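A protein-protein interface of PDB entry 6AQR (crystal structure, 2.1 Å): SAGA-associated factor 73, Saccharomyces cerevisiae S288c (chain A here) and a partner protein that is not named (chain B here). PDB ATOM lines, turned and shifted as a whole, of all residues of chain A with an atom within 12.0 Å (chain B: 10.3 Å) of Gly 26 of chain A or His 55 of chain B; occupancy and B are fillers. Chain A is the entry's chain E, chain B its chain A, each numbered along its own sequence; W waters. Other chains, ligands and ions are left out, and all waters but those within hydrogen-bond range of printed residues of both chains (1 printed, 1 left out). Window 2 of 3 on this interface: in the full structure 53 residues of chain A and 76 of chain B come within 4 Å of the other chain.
O of Gly 52 of chain B is in hydrogen-bond range of N of Ser 28 of chain A. A ring nitrogen (NE2) of His 55 of chain B lies within hydrogen-bond range of the backbone carbonyl oxygen (O) of Gly 26 of chain A, at 2.6 Å.
OG of Ser 28 of chain A sits at hydrogen-bond distance from N of Asp 30 of chain A (3.0 Å). O of Cys 71 of chain B lies within hydrogen-bond range of N of Gly 52 of chain B, at 2.6 Å.
Gly 52 of chain B touches Pro 27 of chain A (O to CA, 3.4 Å). N of Ser 28 of chain A touches CE1 of His 55 of chain B (3.7 Å).
Of chain A, only Gly 26 and Ser 28 come within 4 Å of His 55 of chain B. Of chain B, only Gly 52 (3.4 Å) comes within 4 Å of Pro 27 of chain A. No residue of chain A comes within 4 Å of Cys 51 of chain B. Gly 52 of chain B touches just these residues of chain A: Pro 27 and Ser 28. No residue of chain A comes within 4 Å of Thr 53 of chain B. No residue of chain A comes within 4 Å of Glu 56 of chain B. Printed residues of chain B within 4 Å of Ser 28 of chain A: Gly 52 (2.7 Å) and His 55 (3.7 Å). The nearest residue of chain B that does not touch Gly 26 of chain A is Thr 53 of chain B (4.4 Å).
Of the 23 printed residues of chain B, 2 touch a printed residue of chain A. Hydrophobic or aromatic side chains of chain B that line the printed part of chain A: His 55. Of the 9 printed residues of chain A, 3 touch a printed residue of chain B. Among the printed residues, no Asp or Glu carboxylate lies within 4 Å of a Lys or Arg side-chain nitrogen of the other chain.
Water W1 lies within hydrogen-bond range of the backbone carbonyl oxygen of Leu 46 of chain B (3.0 Å) and the side-chain carboxylate of Asp 30 of chain A (3.3 Å).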
ATOM      1  N   ILE A  11      13.355  18.395   7.299  1.00  0.00           N
ATOM      2  CA  ILE A  11      13.735  19.672   6.655  1.00  0.00           C
ATOM      3  C   ILE A  11      13.231  20.817   7.550  1.00  0.00           C
ATOM      4  O   ILE A  11      12.107  20.720   8.045  1.00  0.00           O
ATOM      5  CB  ILE A  11      13.155  19.729   5.211  1.00  0.00           C
ATOM      6  CG1 ILE A  11      14.009  18.863   4.270  1.00  0.00           C
ATOM      7  CG2 ILE A  11      13.103  21.142   4.666  1.00  0.00           C
ATOM      8  CD1 ILE A  11      13.179  18.012   3.292  1.00  0.00           C
ATOM      9  N   SER A  20       8.054  25.895  -1.327  1.00  0.00           N
ATOM     10  CA  SER A  20       6.894  25.034  -1.633  1.00  0.00           C
ATOM     11  C   SER A  20       7.267  23.553  -1.789  1.00  0.00           C
ATOM     12  O   SER A  20       6.748  22.871  -2.683  1.00  0.00           O
ATOM     13  CB  SER A  20       6.132  25.517  -2.881  1.00  0.00           C
ATOM     14  OG  SER A  20       6.103  26.932  -2.985  1.00  0.00           O
ATOM     15  N   LEU A  21       8.148  23.061  -0.908  1.00  0.00           N
ATOM     16  CA  LEU A  21       8.680  21.689  -0.992  1.00  0.00           C
ATOM     17  C   LEU A  21       7.618  20.645  -0.584  1.00  0.00           C
ATOM     18  O   LEU A  21       6.553  20.528  -1.201  1.00  0.00           O
ATOM     19  CB  LEU A  21       9.964  21.529  -0.127  1.00  0.00           C
ATOM     20  CG  LEU A  21      11.252  22.372  -0.265  1.00  0.00           C
ATOM     21  CD1 LEU A  21      12.333  22.051   0.764  1.00  0.00           C
ATOM     22  CD2 LEU A  21      11.843  22.247  -1.647  1.00  0.00           C
ATOM     23  N   GLY A  26       2.875  10.440  -4.871  1.00  0.00           N
ATOM     24  CA  GLY A  26       2.384   9.815  -6.100  1.00  0.00           C
ATOM     25  C   GLY A  26       3.376   9.962  -7.244  1.00  0.00           C
ATOM     26  O   GLY A  26       4.453  10.520  -7.048  1.00  0.00           O
ATOM     27  N   PRO A  27       3.043   9.441  -8.446  1.00  0.00           N
ATOM     28  CA  PRO A  27       3.930   9.740  -9.585  1.00  0.00           C
ATOM     29  C   PRO A  27       3.576  11.117 -10.197  1.00  0.00           C
ATOM     30  O   PRO A  27       2.487  11.622  -9.936  1.00  0.00           O
ATOM     31  CB  PRO A  27       3.643   8.591 -10.560  1.00  0.00           C
ATOM     32  CG  PRO A  27       2.220   8.170 -10.270  1.00  0.00           C
ATOM     33  CD  PRO A  27       1.903   8.575  -8.840  1.00  0.00           C
ATOM     34  N   SER A  28       4.480  11.698 -10.993  1.00  0.00           N
ATOM     35  CA  SER A  28       4.299  13.038 -11.596  1.00  0.00           C
ATOM     36  C   SER A  28       3.274  13.047 -12.720  1.00  0.00           C
ATOM     37  O   SER A  28       3.014  12.027 -13.323  1.00  0.00           O
ATOM     38  CB  SER A  28       5.663  13.596 -12.098  1.00  0.00           C
ATOM     39  OG  SER A  28       5.552  14.939 -12.546  1.00  0.00           O
ATOM     40  N   ASN A  29       2.672  14.198 -12.976  1.00  0.00           N
ATOM     41  CA  ASN A  29       1.933  14.450 -14.233  1.00  0.00           C
ATOM     42  C   ASN A  29       2.681  15.395 -15.245  1.00  0.00           C
ATOM     43  O   ASN A  29       2.100  15.791 -16.254  1.00  0.00           O
ATOM     44  CB  ASN A  29       0.524  14.997 -13.917  1.00  0.00           C
ATOM     45  CG  ASN A  29       0.565  16.354 -13.193  1.00  0.00           C
ATOM     46  OD1 ASN A  29       1.315  16.552 -12.211  1.00  0.00           O
ATOM     47  ND2 ASN A  29      -0.242  17.297 -13.677  1.00  0.00           N
ATOM     48  N   ASP A  30       3.946  15.759 -14.988  1.00  0.00           N
ATOM     49  CA  ASP A  30       4.654  16.721 -15.867  1.00  0.00           C
ATOM     50  C   ASP A  30       4.897  16.106 -17.235  1.00  0.00           C
ATOM     51  O   ASP A  30       5.058  14.876 -17.353  1.00  0.00           O
ATOM     52  CB  ASP A  30       5.977  17.159 -15.265  1.00  0.00           C
ATOM     53  CG  ASP A  30       5.811  17.937 -13.955  1.00  0.00           C
ATOM     54  OD1 ASP A  30       4.705  18.417 -13.651  1.00  0.00           O
ATOM     55  OD2 ASP A  30       6.808  18.091 -13.218  1.00  0.00           O
ATOM     56  N   SER A  31       4.869  16.958 -18.264  1.00  0.00           N
ATOM     57  CA  SER A  31       5.243  16.562 -19.631  1.00  0.00           C
ATOM     58  C   SER A  31       6.457  17.382 -20.125  1.00  0.00           C
ATOM     59  O   SER A  31       6.446  18.620 -20.049  1.00  0.00           O
ATOM     60  CB  SER A  31       4.063  16.740 -20.565  1.00  0.00           C
ATOM     61  OG  SER A  31       4.477  16.518 -21.896  1.00  0.00           O
ATOM     62  N   PHE B  45      17.255  20.850 -15.139  1.00  0.00           N
ATOM     63  CA  PHE B  45      17.224  19.898 -14.012  1.00  0.00           C
ATOM     64  C   PHE B  45      15.807  19.460 -13.586  1.00  0.00           C
ATOM     65  O   PHE B  45      15.535  18.265 -13.455  1.00  0.00           O
ATOM     66  CB  PHE B  45      17.968  20.458 -12.785  1.00  0.00           C
ATOM     67  CG  PHE B  45      19.465  20.441 -12.916  1.00  0.00           C
ATOM     68  CD1 PHE B  45      20.155  21.614 -12.775  1.00  0.00           C
ATOM     69  CD2 PHE B  45      20.210  19.252 -13.163  1.00  0.00           C
ATOM     70  CE1 PHE B  45      21.559  21.648 -12.918  1.00  0.00           C
ATOM     71  CE2 PHE B  45      21.620  19.292 -13.315  1.00  0.00           C
ATOM     72  CZ  PHE B  45      22.285  20.513 -13.201  1.00  0.00           C
ATOM     73  N   LEU B  46      14.921  20.443 -13.370  1.00  0.00           N
ATOM     74  CA  LEU B  46      13.546  20.184 -12.870  1.00  0.00           C
ATOM     75  C   LEU B  46      12.653  19.520 -13.880  1.00  0.00           C
ATOM     76  O   LEU B  46      11.744  18.772 -13.511  1.00  0.00           O
ATOM     77  CB  LEU B  46      12.856  21.455 -12.334  1.00  0.00           C
ATOM     78  CG  LEU B  46      13.626  22.215 -11.255  1.00  0.00           C
ATOM     79  CD1 LEU B  46      12.925  23.520 -10.881  1.00  0.00           C
ATOM     80  CD2 LEU B  46      13.815  21.366 -10.021  1.00  0.00           C
ATOM     81  N   ASN B  47      12.917  19.752 -15.160  1.00  0.00           N
ATOM     82  CA  ASN B  47      11.982  19.308 -16.206  1.00  0.00           C
ATOM     83  C   ASN B  47      12.478  18.335 -17.225  1.00  0.00           C
ATOM     84  O   ASN B  47      11.672  17.887 -18.083  1.00  0.00           O
ATOM     85  CB  ASN B  47      11.395  20.506 -16.914  1.00  0.00           C
ATOM     86  CG  ASN B  47      10.619  21.408 -15.962  1.00  0.00           C
ATOM     87  OD1 ASN B  47      11.024  22.508 -15.713  1.00  0.00           O
ATOM     88  ND2 ASN B  47       9.585  20.877 -15.349  1.00  0.00           N
ATOM     89  N   THR B  48      13.774  17.984 -17.144  1.00  0.00           N
ATOM     90  CA  THR B  48      14.361  16.948 -18.017  1.00  0.00           C
ATOM     91  C   THR B  48      15.244  15.931 -17.237  1.00  0.00           C
ATOM     92  O   THR B  48      15.547  14.824 -17.745  1.00  0.00           O
ATOM     93  CB  THR B  48      15.132  17.519 -19.279  1.00  0.00           C
ATOM     94  OG1 THR B  48      16.437  17.965 -18.869  1.00  0.00           O
ATOM     95  CG2 THR B  48      14.350  18.680 -19.944  1.00  0.00           C
ATOM     96  N   MET B  49      15.642  16.286 -16.039  1.00  0.00           N
ATOM     97  CA  MET B  49      16.410  15.363 -15.242  1.00  0.00           C
ATOM     98  C   MET B  49      15.744  14.874 -13.928  1.00  0.00           C
ATOM     99  O   MET B  49      16.422  14.410 -13.015  1.00  0.00           O
ATOM    100  CB  MET B  49      17.835  15.919 -15.018  1.00  0.00           C
ATOM    101  CG  MET B  49      18.643  15.947 -16.318  1.00  0.00           C
ATOM    102  SD  MET B  49      20.043  17.055 -16.180  1.00  0.00           S
ATOM    103  CE  MET B  49      20.516  17.251 -17.925  1.00  0.00           C
ATOM    104  N   LYS B  50      14.420  14.928 -13.876  1.00  0.00           N
ATOM    105  CA  LYS B  50      13.723  14.586 -12.680  1.00  0.00           C
ATOM    106  C   LYS B  50      12.797  13.419 -13.003  1.00  0.00           C
ATOM    107  O   LYS B  50      11.976  13.533 -13.873  1.00  0.00           O
ATOM    108  CB  LYS B  50      12.951  15.787 -12.158  1.00  0.00           C
ATOM    109  CG  LYS B  50      12.232  15.531 -10.853  1.00  0.00           C
ATOM    110  CD  LYS B  50      11.237  16.666 -10.625  1.00  0.00           C
ATOM    111  CE  LYS B  50      10.841  16.747  -9.176  1.00  0.00           C
ATOM    112  NZ  LYS B  50       9.658  17.666  -9.066  1.00  0.00           N
ATOM    113  N   CYS B  51      12.952  12.296 -12.310  1.00  0.00           N
ATOM    114  CA  CYS B  51      12.168  11.098 -12.676  1.00  0.00           C
ATOM    115  C   CYS B  51      10.712  11.343 -12.307  1.00  0.00           C
ATOM    116  O   CYS B  51      10.455  11.817 -11.217  1.00  0.00           O
ATOM    117  CB  CYS B  51      12.671   9.901 -11.903  1.00  0.00           C
ATOM    118  SG  CYS B  51      11.972   8.264 -12.309  1.00  0.00           S
ATOM    119  N   GLY B  52       9.788  11.017 -13.217  1.00  0.00           N
ATOM    120  CA  GLY B  52       8.379  11.075 -12.918  1.00  0.00           C
ATOM    121  C   GLY B  52       7.869  10.110 -11.839  1.00  0.00           C
ATOM    122  O   GLY B  52       6.745  10.262 -11.374  1.00  0.00           O
ATOM    123  N   THR B  53       8.654   9.105 -11.464  1.00  0.00           N
ATOM    124  CA  THR B  53       8.174   8.110 -10.499  1.00  0.00           C
ATOM    125  C   THR B  53       8.859   8.292  -9.123  1.00  0.00           C
ATOM    126  O   THR B  53       8.161   8.381  -8.139  1.00  0.00           O
ATOM    127  CB  THR B  53       8.260   6.645 -11.023  1.00  0.00           C
ATOM    128  OG1 THR B  53       9.613   6.228 -11.050  1.00  0.00           O
ATOM    129  CG2 THR B  53       7.696   6.497 -12.418  1.00  0.00           C
ATOM    130  N   CYS B  54      10.198   8.391  -9.038  1.00  0.00           N
ATOM    131  CA  CYS B  54      10.841   8.562  -7.754  1.00  0.00           C
ATOM    132  C   CYS B  54      11.121  10.018  -7.395  1.00  0.00           C
ATOM    133  O   CYS B  54      11.518  10.289  -6.259  1.00  0.00           O
ATOM    134  CB  CYS B  54      12.138   7.729  -7.632  1.00  0.00           C
ATOM    135  SG  CYS B  54      13.487   8.132  -8.804  1.00  0.00           S
ATOM    136  N   HIS B  55      10.968  10.936  -8.365  1.00  0.00           N
ATOM    137  CA  HIS B  55      11.192  12.404  -8.145  1.00  0.00           C
ATOM    138  C   HIS B  55      12.606  12.825  -7.817  1.00  0.00           C
ATOM    139  O   HIS B  55      12.827  13.934  -7.408  1.00  0.00           O
ATOM    140  CB  HIS B  55      10.253  12.967  -7.074  1.00  0.00           C
ATOM    141  CG  HIS B  55       8.835  12.561  -7.281  1.00  0.00           C
ATOM    142  ND1 HIS B  55       8.105  12.946  -8.394  1.00  0.00           N
ATOM    143  CD2 HIS B  55       8.016  11.759  -6.550  1.00  0.00           C
ATOM    144  CE1 HIS B  55       6.887  12.427  -8.327  1.00  0.00           C
ATOM    145  NE2 HIS B  55       6.814  11.689  -7.227  1.00  0.00           N
ATOM    146  N   GLU B  56      13.566  11.945  -7.962  1.00  0.00           N
ATOM    147  CA  GLU B  56      14.949  12.370  -7.738  1.00  0.00           C
ATOM    148  C   GLU B  56      15.565  12.996  -9.024  1.00  0.00           C
ATOM    149  O   GLU B  56      15.219  12.671 -10.201  1.00  0.00           O
ATOM    150  CB  GLU B  56      15.837  11.205  -7.297  1.00  0.00           C
ATOM    151  CG  GLU B  56      15.448  10.422  -6.063  1.00  0.00           C
ATOM    152  CD  GLU B  56      16.517   9.391  -5.778  1.00  0.00           C
ATOM    153  OE1 GLU B  56      17.692   9.804  -5.892  1.00  0.00           O
ATOM    154  OE2 GLU B  56      16.214   8.187  -5.505  1.00  0.00           O
ATOM    155  N   ILE B  57      16.493  13.892  -8.782  1.00  0.00           N
ATOM    156  CA  ILE B  57      17.225  14.532  -9.843  1.00  0.00           C
ATOM    157  C   ILE B  57      18.473  13.731 -10.081  1.00  0.00           C
ATOM    158  O   ILE B  57      19.153  13.341  -9.124  1.00  0.00           O
ATOM    159  CB  ILE B  57      17.491  16.004  -9.471  1.00  0.00           C
ATOM    160  CG1 ILE B  57      16.106  16.717  -9.483  1.00  0.00           C
ATOM    161  CG2 ILE B  57      18.479  16.620 -10.488  1.00  0.00           C
ATOM    162  CD1 ILE B  57      16.056  17.877  -8.563  1.00  0.00           C
ATOM    163  N   ASN B  58      18.765  13.461 -11.364  1.00  0.00           N
ATOM    164  CA  ASN B  58      19.985  12.728 -11.743  1.00  0.00           C
ATOM    165  C   ASN B  58      20.132  11.375 -11.050  1.00  0.00           C
ATOM    166  O   ASN B  58      21.228  11.010 -10.585  1.00  0.00           O
ATOM    167  CB  ASN B  58      21.235  13.564 -11.468  1.00  0.00           C
ATOM    168  CG  ASN B  58      21.389  14.753 -12.395  1.00  0.00           C
ATOM    169  OD1 ASN B  58      20.956  14.742 -13.562  1.00  0.00           O
ATOM    170  ND2 ASN B  58      22.100  15.775 -11.892  1.00  0.00           N
ATOM    171  N   SER B  59      19.055  10.598 -11.006  1.00  0.00           N
ATOM    172  CA  SER B  59      19.123   9.208 -10.543  1.00  0.00           C
ATOM    173  C   SER B  59      19.699   8.370 -11.650  1.00  0.00           C
ATOM    174  O   SER B  59      18.987   7.559 -12.309  1.00  0.00           O
ATOM    175  CB  SER B  59      17.690   8.727 -10.142  1.00  0.00           C
ATOM    176  OG  SER B  59      17.735   7.419  -9.639  1.00  0.00           O
ATOM    177  N   GLY B  60      20.983   8.615 -11.936  1.00  0.00           N
ATOM    178  CA  GLY B  60      21.583   8.208 -13.246  1.00  0.00           C
ATOM    179  C   GLY B  60      21.014   9.047 -14.423  1.00  0.00           C
ATOM    180  O   GLY B  60      20.439  10.097 -14.225  1.00  0.00           O
ATOM    181  N   THR B  62      18.468  10.337 -17.065  1.00  0.00           N
ATOM    182  CA  THR B  62      17.008  10.442 -17.138  1.00  0.00           C
ATOM    183  C   THR B  62      16.646  10.496 -18.583  1.00  0.00           C
ATOM    184  O   THR B  62      17.283  11.234 -19.332  1.00  0.00           O
ATOM    185  CB  THR B  62      16.528  11.713 -16.399  1.00  0.00           C
ATOM    186  OG1 THR B  62      17.192  11.814 -15.121  1.00  0.00           O
ATOM    187  CG2 THR B  62      15.030  11.674 -16.176  1.00  0.00           C
ATOM    188  N   PHE B  70       6.418  11.751 -20.172  1.00  0.00           N
ATOM    189  CA  PHE B  70       7.052  11.246 -18.943  1.00  0.00           C
ATOM    190  C   PHE B  70       8.605  11.205 -19.036  1.00  0.00           C
ATOM    191  O   PHE B  70       9.112  10.983 -20.102  1.00  0.00           O
ATOM    192  CB  PHE B  70       6.405   9.888 -18.598  1.00  0.00           C
ATOM    193  CG  PHE B  70       7.182   9.046 -17.661  1.00  0.00           C
ATOM    194  CD1 PHE B  70       8.174   8.191 -18.184  1.00  0.00           C
ATOM    195  CD2 PHE B  70       6.887   8.996 -16.286  1.00  0.00           C
ATOM    196  CE1 PHE B  70       8.923   7.380 -17.361  1.00  0.00           C
ATOM    197  CE2 PHE B  70       7.642   8.156 -15.432  1.00  0.00           C
ATOM    198  CZ  PHE B  70       8.672   7.351 -15.970  1.00  0.00           C
ATOM    199  N   CYS B  71       9.327  11.458 -17.936  1.00  0.00           N
ATOM    200  CA  CYS B  71      10.775  11.220 -17.850  1.00  0.00           C
ATOM    201  C   CYS B  71      11.007  10.202 -16.755  1.00  0.00           C
ATOM    202  O   CYS B  71      10.392  10.318 -15.696  1.00  0.00           O
ATOM    203  CB  CYS B  71      11.553  12.498 -17.463  1.00  0.00           C
ATOM    204  SG  CYS B  71      11.295  13.884 -18.570  1.00  0.00           S
ATOM    205  N   GLY B  72      11.880   9.219 -17.006  1.00  0.00           N
ATOM    206  CA  GLY B  72      12.250   8.247 -16.025  1.00  0.00           C
ATOM    207  C   GLY B  72      13.724   7.987 -15.908  1.00  0.00           C
ATOM    208  O   GLY B  72      14.427   8.086 -16.895  1.00  0.00           O
ATOM    209  N   CYS B  73      14.153   7.632 -14.713  1.00  0.00           N
ATOM    210  CA  CYS B  73      15.520   7.392 -14.393  1.00  0.00           C
ATOM    211  C   CYS B  73      16.086   6.011 -14.816  1.00  0.00           C
ATOM    212  O   CYS B  73      15.329   5.023 -15.081  1.00  0.00           O
ATOM    213  CB  CYS B  73      15.740   7.592 -12.879  1.00  0.00           C
ATOM    214  SG  CYS B  73      15.182   6.260 -11.730  1.00  0.00           S
ATOM    215  N   HIS B  76      17.062   3.450 -10.727  1.00  0.00           N
ATOM    216  CA  HIS B  76      15.993   2.690 -10.128  1.00  0.00           C
ATOM    217  C   HIS B  76      15.114   2.023 -11.146  1.00  0.00           C
ATOM    218  O   HIS B  76      14.033   1.618 -10.817  1.00  0.00           O
ATOM    219  CB  HIS B  76      15.120   3.588  -9.226  1.00  0.00           C
ATOM    220  CG  HIS B  76      15.883   4.300  -8.152  1.00  0.00           C
ATOM    221  ND1 HIS B  76      16.889   3.696  -7.428  1.00  0.00           N
ATOM    222  CD2 HIS B  76      15.782   5.566  -7.670  1.00  0.00           C
ATOM    223  CE1 HIS B  76      17.395   4.560  -6.559  1.00  0.00           C
ATOM    224  NE2 HIS B  76      16.731   5.697  -6.673  1.00  0.00           N
ATOM    225  N   HIS B  78      13.369   3.074 -13.581  1.00  0.00           N
ATOM    226  CA  HIS B  78      12.065   3.666 -13.725  1.00  0.00           C
ATOM    227  C   HIS B  78      11.633   3.909 -15.159  1.00  0.00           C
ATOM    228  O   HIS B  78      10.427   3.835 -15.469  1.00  0.00           O
ATOM    229  CB  HIS B  78      11.850   4.893 -12.787  1.00  0.00           C
ATOM    230  CG  HIS B  78      11.807   4.548 -11.329  1.00  0.00           C
ATOM    231  ND1 HIS B  78      12.186   5.435 -10.347  1.00  0.00           N
ATOM    232  CD2 HIS B  78      11.423   3.415 -10.682  1.00  0.00           C
ATOM    233  CE1 HIS B  78      12.054   4.873  -9.159  1.00  0.00           C
ATOM    234  NE2 HIS B  78      11.603   3.639  -9.337  1.00  0.00           N
HETATM  235  O   HOH W   1       9.595  16.966 -14.555  1.00  0.00           O
